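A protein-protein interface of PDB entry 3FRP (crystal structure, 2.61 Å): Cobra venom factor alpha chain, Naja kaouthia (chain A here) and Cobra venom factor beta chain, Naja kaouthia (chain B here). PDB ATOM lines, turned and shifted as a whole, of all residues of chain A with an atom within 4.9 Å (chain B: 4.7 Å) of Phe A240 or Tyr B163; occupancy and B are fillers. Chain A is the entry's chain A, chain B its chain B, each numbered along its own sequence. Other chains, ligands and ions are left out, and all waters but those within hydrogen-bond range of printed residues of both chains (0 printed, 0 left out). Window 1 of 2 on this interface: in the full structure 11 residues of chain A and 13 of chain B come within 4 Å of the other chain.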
ATOM      1  N   VAL A 238      17.630 -14.367  17.403  1.00  0.00           N
ATOM      2  CA  VAL A 238      18.713 -13.830  16.574  1.00  0.00           C
ATOM      3  C   VAL A 238      18.346 -12.466  15.996  1.00  0.00           C
ATOM      4  O   VAL A 238      17.175 -12.134  15.889  1.00  0.00           O
ATOM      5  CB  VAL A 238      19.081 -14.792  15.408  1.00  0.00           C
ATOM      6  CG1 VAL A 238      19.192 -16.238  15.893  1.00  0.00           C
ATOM      7  CG2 VAL A 238      18.058 -14.684  14.305  1.00  0.00           C
ATOM      8  N   ALA A 239      19.359 -11.686  15.615  1.00  0.00           N
ATOM      9  CA  ALA A 239      19.129 -10.382  14.988  1.00  0.00           C
ATOM     10  C   ALA A 239      19.862 -10.216  13.641  1.00  0.00           C
ATOM     11  O   ALA A 239      20.934 -10.791  13.420  1.00  0.00           O
ATOM     12  CB  ALA A 239      19.457  -9.228  15.963  1.00  0.00           C
ATOM     13  N   PHE A 240      19.249  -9.440  12.746  1.00  0.00           N
ATOM     14  CA  PHE A 240      19.828  -9.118  11.446  1.00  0.00           C
ATOM     15  C   PHE A 240      20.012  -7.612  11.383  1.00  0.00           C
ATOM     16  O   PHE A 240      19.047  -6.851  11.510  1.00  0.00           O
ATOM     17  CB  PHE A 240      18.917  -9.585  10.310  1.00  0.00           C
ATOM     18  CG  PHE A 240      18.691 -11.081  10.276  1.00  0.00           C
ATOM     19  CD1 PHE A 240      17.550 -11.636  10.850  1.00  0.00           C
ATOM     20  CD2 PHE A 240      19.610 -11.932   9.649  1.00  0.00           C
ATOM     21  CE1 PHE A 240      17.328 -13.006  10.810  1.00  0.00           C
ATOM     22  CE2 PHE A 240      19.398 -13.316   9.605  1.00  0.00           C
ATOM     23  CZ  PHE A 240      18.257 -13.850  10.192  1.00  0.00           C
ATOM     24  N   VAL A 241      21.263  -7.189  11.220  1.00  0.00           N
ATOM     25  CA  VAL A 241      21.606  -5.776  11.182  1.00  0.00           C
ATOM     26  C   VAL A 241      22.306  -5.479   9.889  1.00  0.00           C
ATOM     27  O   VAL A 241      23.216  -6.216   9.479  1.00  0.00           O
ATOM     28  CB  VAL A 241      22.550  -5.375  12.326  1.00  0.00           C
ATOM     29  CG1 VAL A 241      22.831  -3.891  12.276  1.00  0.00           C
ATOM     30  CG2 VAL A 241      21.958  -5.781  13.676  1.00  0.00           C
ATOM     31  N   LEU A 242      21.874  -4.390   9.258  1.00  0.00           N
ATOM     32  CA  LEU A 242      22.474  -3.890   8.040  1.00  0.00           C
ATOM     33  C   LEU A 242      22.740  -2.405   8.259  1.00  0.00           C
ATOM     34  O   LEU A 242      21.860  -1.674   8.725  1.00  0.00           O
ATOM     35  CB  LEU A 242      21.500  -4.117   6.875  1.00  0.00           C
ATOM     36  CG  LEU A 242      21.786  -3.479   5.506  1.00  0.00           C
ATOM     37  CD1 LEU A 242      22.741  -4.338   4.699  1.00  0.00           C
ATOM     38  CD2 LEU A 242      20.482  -3.253   4.757  1.00  0.00           C
ATOM     39  N   THR A 259      25.014  -8.805   8.937  1.00  0.00           N
ATOM     40  CA  THR A 259      25.415  -9.892   9.812  1.00  0.00           C
ATOM     41  C   THR A 259      24.240 -10.384  10.653  1.00  0.00           C
ATOM     42  O   THR A 259      23.345  -9.609  11.018  1.00  0.00           O
ATOM     43  CB  THR A 259      26.614  -9.544  10.741  1.00  0.00           C
ATOM     44  OG1 THR A 259      26.409  -8.275  11.366  1.00  0.00           O
ATOM     45  CG2 THR A 259      27.936  -9.538   9.972  1.00  0.00           C
ATOM     46  N   ARG A 260      24.261 -11.685  10.940  1.00  0.00           N
ATOM     47  CA  ARG A 260      23.306 -12.319  11.815  1.00  0.00           C
ATOM     48  C   ARG A 260      24.002 -12.647  13.125  1.00  0.00           C
ATOM     49  O   ARG A 260      24.971 -13.395  13.157  1.00  0.00           O
ATOM     50  CB  ARG A 260      22.759 -13.590  11.169  1.00  0.00           C
ATOM     51  CG  ARG A 260      21.761 -14.328  12.024  1.00  0.00           C
ATOM     52  CD  ARG A 260      21.505 -15.734  11.515  1.00  0.00           C
ATOM     53  NE  ARG A 260      22.744 -16.493  11.381  1.00  0.00           N
ATOM     54  CZ  ARG A 260      23.174 -17.051  10.251  1.00  0.00           C
ATOM     55  NH1 ARG A 260      22.455 -16.992   9.126  1.00  0.00           N
ATOM     56  NH2 ARG A 260      24.322 -17.704  10.263  1.00  0.00           N
ATOM     57  N   SER A 295      19.928  -0.706  10.630  1.00  0.00           N
ATOM     58  CA  SER A 295      18.601  -1.267  10.630  1.00  0.00           C
ATOM     59  C   SER A 295      18.653  -2.639  11.272  1.00  0.00           C
ATOM     60  O   SER A 295      19.471  -3.483  10.884  1.00  0.00           O
ATOM     61  CB  SER A 295      18.080  -1.371   9.212  1.00  0.00           C
ATOM     62  OG  SER A 295      16.695  -1.638   9.253  1.00  0.00           O
ATOM     63  N   VAL A 296      17.783  -2.855  12.252  1.00  0.00           N
ATOM     64  CA  VAL A 296      17.882  -4.026  13.107  1.00  0.00           C
ATOM     65  C   VAL A 296      16.546  -4.755  13.215  1.00  0.00           C
ATOM     66  O   VAL A 296      15.497  -4.170  13.494  1.00  0.00           O
ATOM     67  CB  VAL A 296      18.533  -3.660  14.491  1.00  0.00           C
ATOM     68  CG1 VAL A 296      17.716  -2.624  15.186  1.00  0.00           C
ATOM     69  CG2 VAL A 296      18.680  -4.858  15.379  1.00  0.00           C
ATOM     70  N   THR A 297      16.611  -6.050  12.954  1.00  0.00           N
ATOM     71  CA  THR A 297      15.444  -6.911  12.858  1.00  0.00           C
ATOM     72  C   THR A 297      15.660  -8.068  13.810  1.00  0.00           C
ATOM     73  O   THR A 297      16.527  -8.909  13.561  1.00  0.00           O
ATOM     74  CB  THR A 297      15.305  -7.450  11.421  1.00  0.00           C
ATOM     75  OG1 THR A 297      15.200  -6.347  10.527  1.00  0.00           O
ATOM     76  CG2 THR A 297      14.069  -8.322  11.263  1.00  0.00           C
ATOM     77  N   MET A 299      14.205 -11.423  15.864  1.00  0.00           N
ATOM     78  CA  MET A 299      13.267 -12.526  15.774  1.00  0.00           C
ATOM     79  C   MET A 299      13.373 -13.437  17.030  1.00  0.00           C
ATOM     80  O   MET A 299      14.488 -13.803  17.448  1.00  0.00           O
ATOM     81  CB  MET A 299      13.577 -13.312  14.500  1.00  0.00           C
ATOM     82  CG  MET A 299      12.600 -14.396  14.189  1.00  0.00           C
ATOM     83  SD  MET A 299      13.121 -15.393  12.776  1.00  0.00           S
ATOM     84  CE  MET A 299      11.824 -16.638  12.815  1.00  0.00           C
ATOM     85  N   THR A 300      12.222 -13.783  17.629  1.00  0.00           N
ATOM     86  CA  THR A 300      12.191 -14.756  18.752  1.00  0.00           C
ATOM     87  C   THR A 300      12.672 -16.150  18.305  1.00  0.00           C
ATOM     88  O   THR A 300      12.481 -16.541  17.153  1.00  0.00           O
ATOM     89  CB  THR A 300      10.810 -14.853  19.466  1.00  0.00           C
ATOM     90  OG1 THR A 300       9.822 -15.339  18.560  1.00  0.00           O
ATOM     91  CG2 THR A 300      10.364 -13.517  19.999  1.00  0.00           C
ATOM     92  N   MET B 116      21.197 -15.017   3.646  1.00  0.00           N
ATOM     93  CA  MET B 116      20.675 -15.028   5.008  1.00  0.00           C
ATOM     94  C   MET B 116      19.232 -15.553   5.011  1.00  0.00           C
ATOM     95  O   MET B 116      18.293 -14.895   5.458  1.00  0.00           O
ATOM     96  CB  MET B 116      20.813 -13.625   5.621  1.00  0.00           C
ATOM     97  CG  MET B 116      21.434 -13.597   7.020  1.00  0.00           C
ATOM     98  SD  MET B 116      23.191 -13.973   7.129  1.00  0.00           S
ATOM     99  CE  MET B 116      23.898 -12.364   6.816  1.00  0.00           C
ATOM    100  N   THR B 117      19.080 -16.756   4.475  1.00  0.00           N
ATOM    101  CA  THR B 117      17.800 -17.430   4.431  1.00  0.00           C
ATOM    102  C   THR B 117      17.546 -18.337   5.656  1.00  0.00           C
ATOM    103  O   THR B 117      18.487 -18.773   6.341  1.00  0.00           O
ATOM    104  CB  THR B 117      17.589 -18.146   3.045  1.00  0.00           C
ATOM    105  OG1 THR B 117      16.988 -19.439   3.219  1.00  0.00           O
ATOM    106  CG2 THR B 117      18.907 -18.279   2.286  1.00  0.00           C
ATOM    107  N   ILE B 118      16.267 -18.586   5.924  1.00  0.00           N
ATOM    108  CA  ILE B 118      15.810 -19.197   7.162  1.00  0.00           C
ATOM    109  C   ILE B 118      14.848 -20.360   6.887  1.00  0.00           C
ATOM    110  O   ILE B 118      13.898 -20.225   6.121  1.00  0.00           O
ATOM    111  CB  ILE B 118      15.097 -18.149   8.039  1.00  0.00           C
ATOM    112  CG1 ILE B 118      16.055 -17.003   8.387  1.00  0.00           C
ATOM    113  CG2 ILE B 118      14.536 -18.777   9.316  1.00  0.00           C
ATOM    114  CD1 ILE B 118      15.389 -15.784   8.965  1.00  0.00           C
ATOM    115  N   ASP B 142      28.434 -22.751   7.299  1.00  0.00           N
ATOM    116  CA  ASP B 142      27.514 -21.651   7.127  1.00  0.00           C
ATOM    117  C   ASP B 142      26.144 -22.035   7.699  1.00  0.00           C
ATOM    118  O   ASP B 142      25.217 -22.352   6.939  1.00  0.00           O
ATOM    119  CB  ASP B 142      27.391 -21.314   5.631  1.00  0.00           C
ATOM    120  CG  ASP B 142      28.648 -20.641   5.058  1.00  0.00           C
ATOM    121  OD1 ASP B 142      29.115 -19.630   5.636  1.00  0.00           O
ATOM    122  OD2 ASP B 142      29.158 -21.117   4.013  1.00  0.00           O
ATOM    123  N   ARG B 143      26.027 -22.020   9.031  1.00  0.00           N
ATOM    124  CA  ARG B 143      24.773 -22.356   9.723  1.00  0.00           C
ATOM    125  C   ARG B 143      24.732 -21.853  11.172  1.00  0.00           C
ATOM    126  O   ARG B 143      25.769 -21.527  11.744  1.00  0.00           O
ATOM    127  CB  ARG B 143      24.510 -23.873   9.688  1.00  0.00           C
ATOM    128  CG  ARG B 143      23.768 -24.340   8.443  1.00  0.00           C
ATOM    129  CD  ARG B 143      23.085 -25.676   8.634  1.00  0.00           C
ATOM    130  NE  ARG B 143      23.995 -26.796   8.441  1.00  0.00           N
ATOM    131  CZ  ARG B 143      24.250 -27.369   7.270  1.00  0.00           C
ATOM    132  NH1 ARG B 143      23.673 -26.926   6.154  1.00  0.00           N
ATOM    133  NH2 ARG B 143      25.090 -28.393   7.215  1.00  0.00           N
ATOM    134  N   TYR B 144      23.534 -21.781  11.750  1.00  0.00           N
ATOM    135  CA  TYR B 144      23.354 -21.494  13.174  1.00  0.00           C
ATOM    136  C   TYR B 144      22.025 -22.031  13.673  1.00  0.00           C
ATOM    137  O   TYR B 144      21.013 -21.951  12.977  1.00  0.00           O
ATOM    138  CB  TYR B 144      23.447 -19.991  13.477  1.00  0.00           C
ATOM    139  CG  TYR B 144      23.180 -19.606  14.937  1.00  0.00           C
ATOM    140  CD1 TYR B 144      24.066 -19.971  15.960  1.00  0.00           C
ATOM    141  CD2 TYR B 144      22.051 -18.863  15.288  1.00  0.00           C
ATOM    142  CE1 TYR B 144      23.823 -19.617  17.283  1.00  0.00           C
ATOM    143  CE2 TYR B 144      21.803 -18.506  16.608  1.00  0.00           C
ATOM    144  CZ  TYR B 144      22.691 -18.881  17.595  1.00  0.00           C
ATOM    145  OH  TYR B 144      22.440 -18.510  18.896  1.00  0.00           O
ATOM    146  N   ILE B 161      14.515 -23.784  14.231  1.00  0.00           N
ATOM    147  CA  ILE B 161      14.853 -22.855  13.156  1.00  0.00           C
ATOM    148  C   ILE B 161      16.326 -22.945  12.821  1.00  0.00           C
ATOM    149  O   ILE B 161      17.172 -22.777  13.700  1.00  0.00           O
ATOM    150  CB  ILE B 161      14.438 -21.413  13.525  1.00  0.00           C
ATOM    151  CG1 ILE B 161      12.912 -21.292  13.419  1.00  0.00           C
ATOM    152  CG2 ILE B 161      15.074 -20.408  12.603  1.00  0.00           C
ATOM    153  CD1 ILE B 161      12.263 -20.507  14.532  1.00  0.00           C
ATOM    154  N   ILE B 162      16.621 -23.229  11.551  1.00  0.00           N
ATOM    155  CA  ILE B 162      17.997 -23.297  11.068  1.00  0.00           C
ATOM    156  C   ILE B 162      18.317 -22.055  10.244  1.00  0.00           C
ATOM    157  O   ILE B 162      17.608 -21.752   9.273  1.00  0.00           O
ATOM    158  CB  ILE B 162      18.263 -24.592  10.231  1.00  0.00           C
ATOM    159  CG1 ILE B 162      18.281 -25.838  11.128  1.00  0.00           C
ATOM    160  CG2 ILE B 162      19.600 -24.527   9.516  1.00  0.00           C
ATOM    161  CD1 ILE B 162      17.241 -26.903  10.784  1.00  0.00           C
ATOM    162  N   TYR B 163      19.381 -21.341  10.608  1.00  0.00           N
ATOM    163  CA  TYR B 163      19.801 -20.162   9.834  1.00  0.00           C
ATOM    164  C   TYR B 163      20.936 -20.455   8.880  1.00  0.00           C
ATOM    165  O   TYR B 163      21.970 -20.987   9.278  1.00  0.00           O
ATOM    166  CB  TYR B 163      20.215 -19.033  10.751  1.00  0.00           C
ATOM    167  CG  TYR B 163      19.144 -18.644  11.731  1.00  0.00           C
ATOM    168  CD1 TYR B 163      18.253 -17.613  11.451  1.00  0.00           C
ATOM    169  CD2 TYR B 163      19.027 -19.307  12.947  1.00  0.00           C
ATOM    170  CE1 TYR B 163      17.267 -17.269  12.366  1.00  0.00           C
ATOM    171  CE2 TYR B 163      18.070 -18.963  13.853  1.00  0.00           C
ATOM    172  CZ  TYR B 163      17.191 -17.950  13.574  1.00  0.00           C
ATOM    173  OH  TYR B 163      16.236 -17.637  14.514  1.00  0.00           O
ATOM    174  N   LEU B 164      20.740 -20.109   7.615  1.00  0.00           N
ATOM    175  CA  LEU B 164      21.770 -20.345   6.623  1.00  0.00           C
ATOM    176  C   LEU B 164      22.253 -19.009   6.052  1.00  0.00           C
ATOM    177  O   LEU B 164      21.459 -18.092   5.889  1.00  0.00           O
ATOM    178  CB  LEU B 164      21.244 -21.274   5.523  1.00  0.00           C
ATOM    179  CG  LEU B 164      20.992 -22.751   5.877  1.00  0.00           C
ATOM    180  CD1 LEU B 164      19.581 -22.946   6.380  1.00  0.00           C
ATOM    181  CD2 LEU B 164      21.233 -23.679   4.682  1.00  0.00           C
ATOM    182  N   ASN B 165      23.547 -18.895   5.772  1.00  0.00           N
ATOM    183  CA  ASN B 165      24.076 -17.694   5.138  1.00  0.00           C
ATOM    184  C   ASN B 165      23.618 -17.542   3.691  1.00  0.00           C
ATOM    185  O   ASN B 165      23.208 -16.466   3.282  1.00  0.00           O
ATOM    186  CB  ASN B 165      25.601 -17.665   5.224  1.00  0.00           C
ATOM    187  CG  ASN B 165      26.099 -17.576   6.651  1.00  0.00           C
ATOM    188  OD1 ASN B 165      25.451 -16.978   7.518  1.00  0.00           O
ATOM    189  ND2 ASN B 165      27.244 -18.180   6.909  1.00  0.00           N
ATOM    190  N   TYR B 198      16.329 -12.729   4.302  1.00  0.00           N
ATOM    191  CA  TYR B 198      16.362 -11.371   4.864  1.00  0.00           C
ATOM    192  C   TYR B 198      15.680 -10.283   4.033  1.00  0.00           C
ATOM    193  O   TYR B 198      14.932  -9.467   4.571  1.00  0.00           O
ATOM    194  CB  TYR B 198      17.793 -10.929   5.156  1.00  0.00           C
ATOM    195  CG  TYR B 198      17.835  -9.506   5.661  1.00  0.00           C
ATOM    196  CD1 TYR B 198      18.097  -8.428   4.800  1.00  0.00           C
ATOM    197  CD2 TYR B 198      17.579  -9.231   6.997  1.00  0.00           C
ATOM    198  CE1 TYR B 198      18.088  -7.116   5.276  1.00  0.00           C
ATOM    199  CE2 TYR B 198      17.577  -7.936   7.479  1.00  0.00           C
ATOM    200  CZ  TYR B 198      17.832  -6.885   6.631  1.00  0.00           C
ATOM    201  OH  TYR B 198      17.826  -5.622   7.171  1.00  0.00           O
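CE2 of Tyr B144 touches CG1 of Val A238 (3.5 Å).
Val A238 touches Tyr B163 (CG2 to CE1, 3.3 Å).
Met B116 touches Phe A240 (CG to CE2, 3.3 Å).
Phe A240 touches Ile B118.
Phe A240 touches Tyr B163 (CZ to CD1, 3.97 Å).
Phe A240 touches Tyr B198.
Leu A242 touches Tyr B198.
CB of Tyr B163 touches NH1 of Arg A260, 3.4 Å away.
Leu B164 touches Arg A260 (O to NH1, 3.6 Å).
Of the printed residues of chain B, Phe A240 touches Met B116, Ile B118, Tyr B163 and Tyr B198.
Tyr B163 touches just these residues of chain A: Val A238 (3.3 Å), Phe A240 (3.97 Å) and Arg A260 (3.4 Å).
Printed residues of chain B within 4 Å of Leu A242: Tyr B198 (3.98 Å).
Printed residues of chain B within 4 Å of Val A238: Tyr B144 (3.5 Å) and Tyr B163 (3.3 Å).
Of the printed residues of chain B, Arg A260 touches Met B116 (3.7 Å), Tyr B163 (3.4 Å), Leu B164 (3.6 Å) and Asn B165 (3.1 Å).
The nearest printed residue of chain B that does not touch Phe A240 is Thr B117 (6.2 Å).
The nearest printed residue of chain B that does not touch Arg A260 is Tyr B144 (4.04 Å).
NH2 of Arg A260 sits at hydrogen-bond distance from OD1 of Asn B165 (3.1 Å).
NH1 of Arg A260 sits at hydrogen-bond distance from SD of Met B116 (3.7 Å).
Of the 12 printed residues of chain A, 4 touch a printed residue of chain B.
Hydrophobic or aromatic side chains of chain B that line the printed part of chain A: Met B116, Ile B118, Tyr B144, Tyr B163 and Tyr B198.
Among the printed residues, 11 pairs touch across the chains.
Among the printed residues, no Asp or Glu carboxylate lies within 4 Å of a Lys or Arg side-chain nitrogen of the other chain.
The backbone carbonyl oxygen (O) of Leu A242 lies within hydrogen-bond range of the backbone NH (N) of Ser A295.
The backbone carbonyl oxygen (O) of Tyr B144 lies within hydrogen-bond range of the backbone NH (N) of Tyr B163 (2.9 Å).
The backbone carbonyl oxygen (O) of Thr A297 sits at hydrogen-bond distance from the backbone NH (N) of Phe A240 (2.9 Å).
The side-chain amide nitrogen (ND2) of Asn B165 lies within hydrogen-bond range of the side-chain carboxylate (OD1) of Asp B142.
The backbone carbonyl oxygen (O) of Thr B117 lies within hydrogen-bond range of the backbone NH (N) of Leu B164.
O of Val A238 sits at hydrogen-bond distance from N of Met A299, 3.1 Å away.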
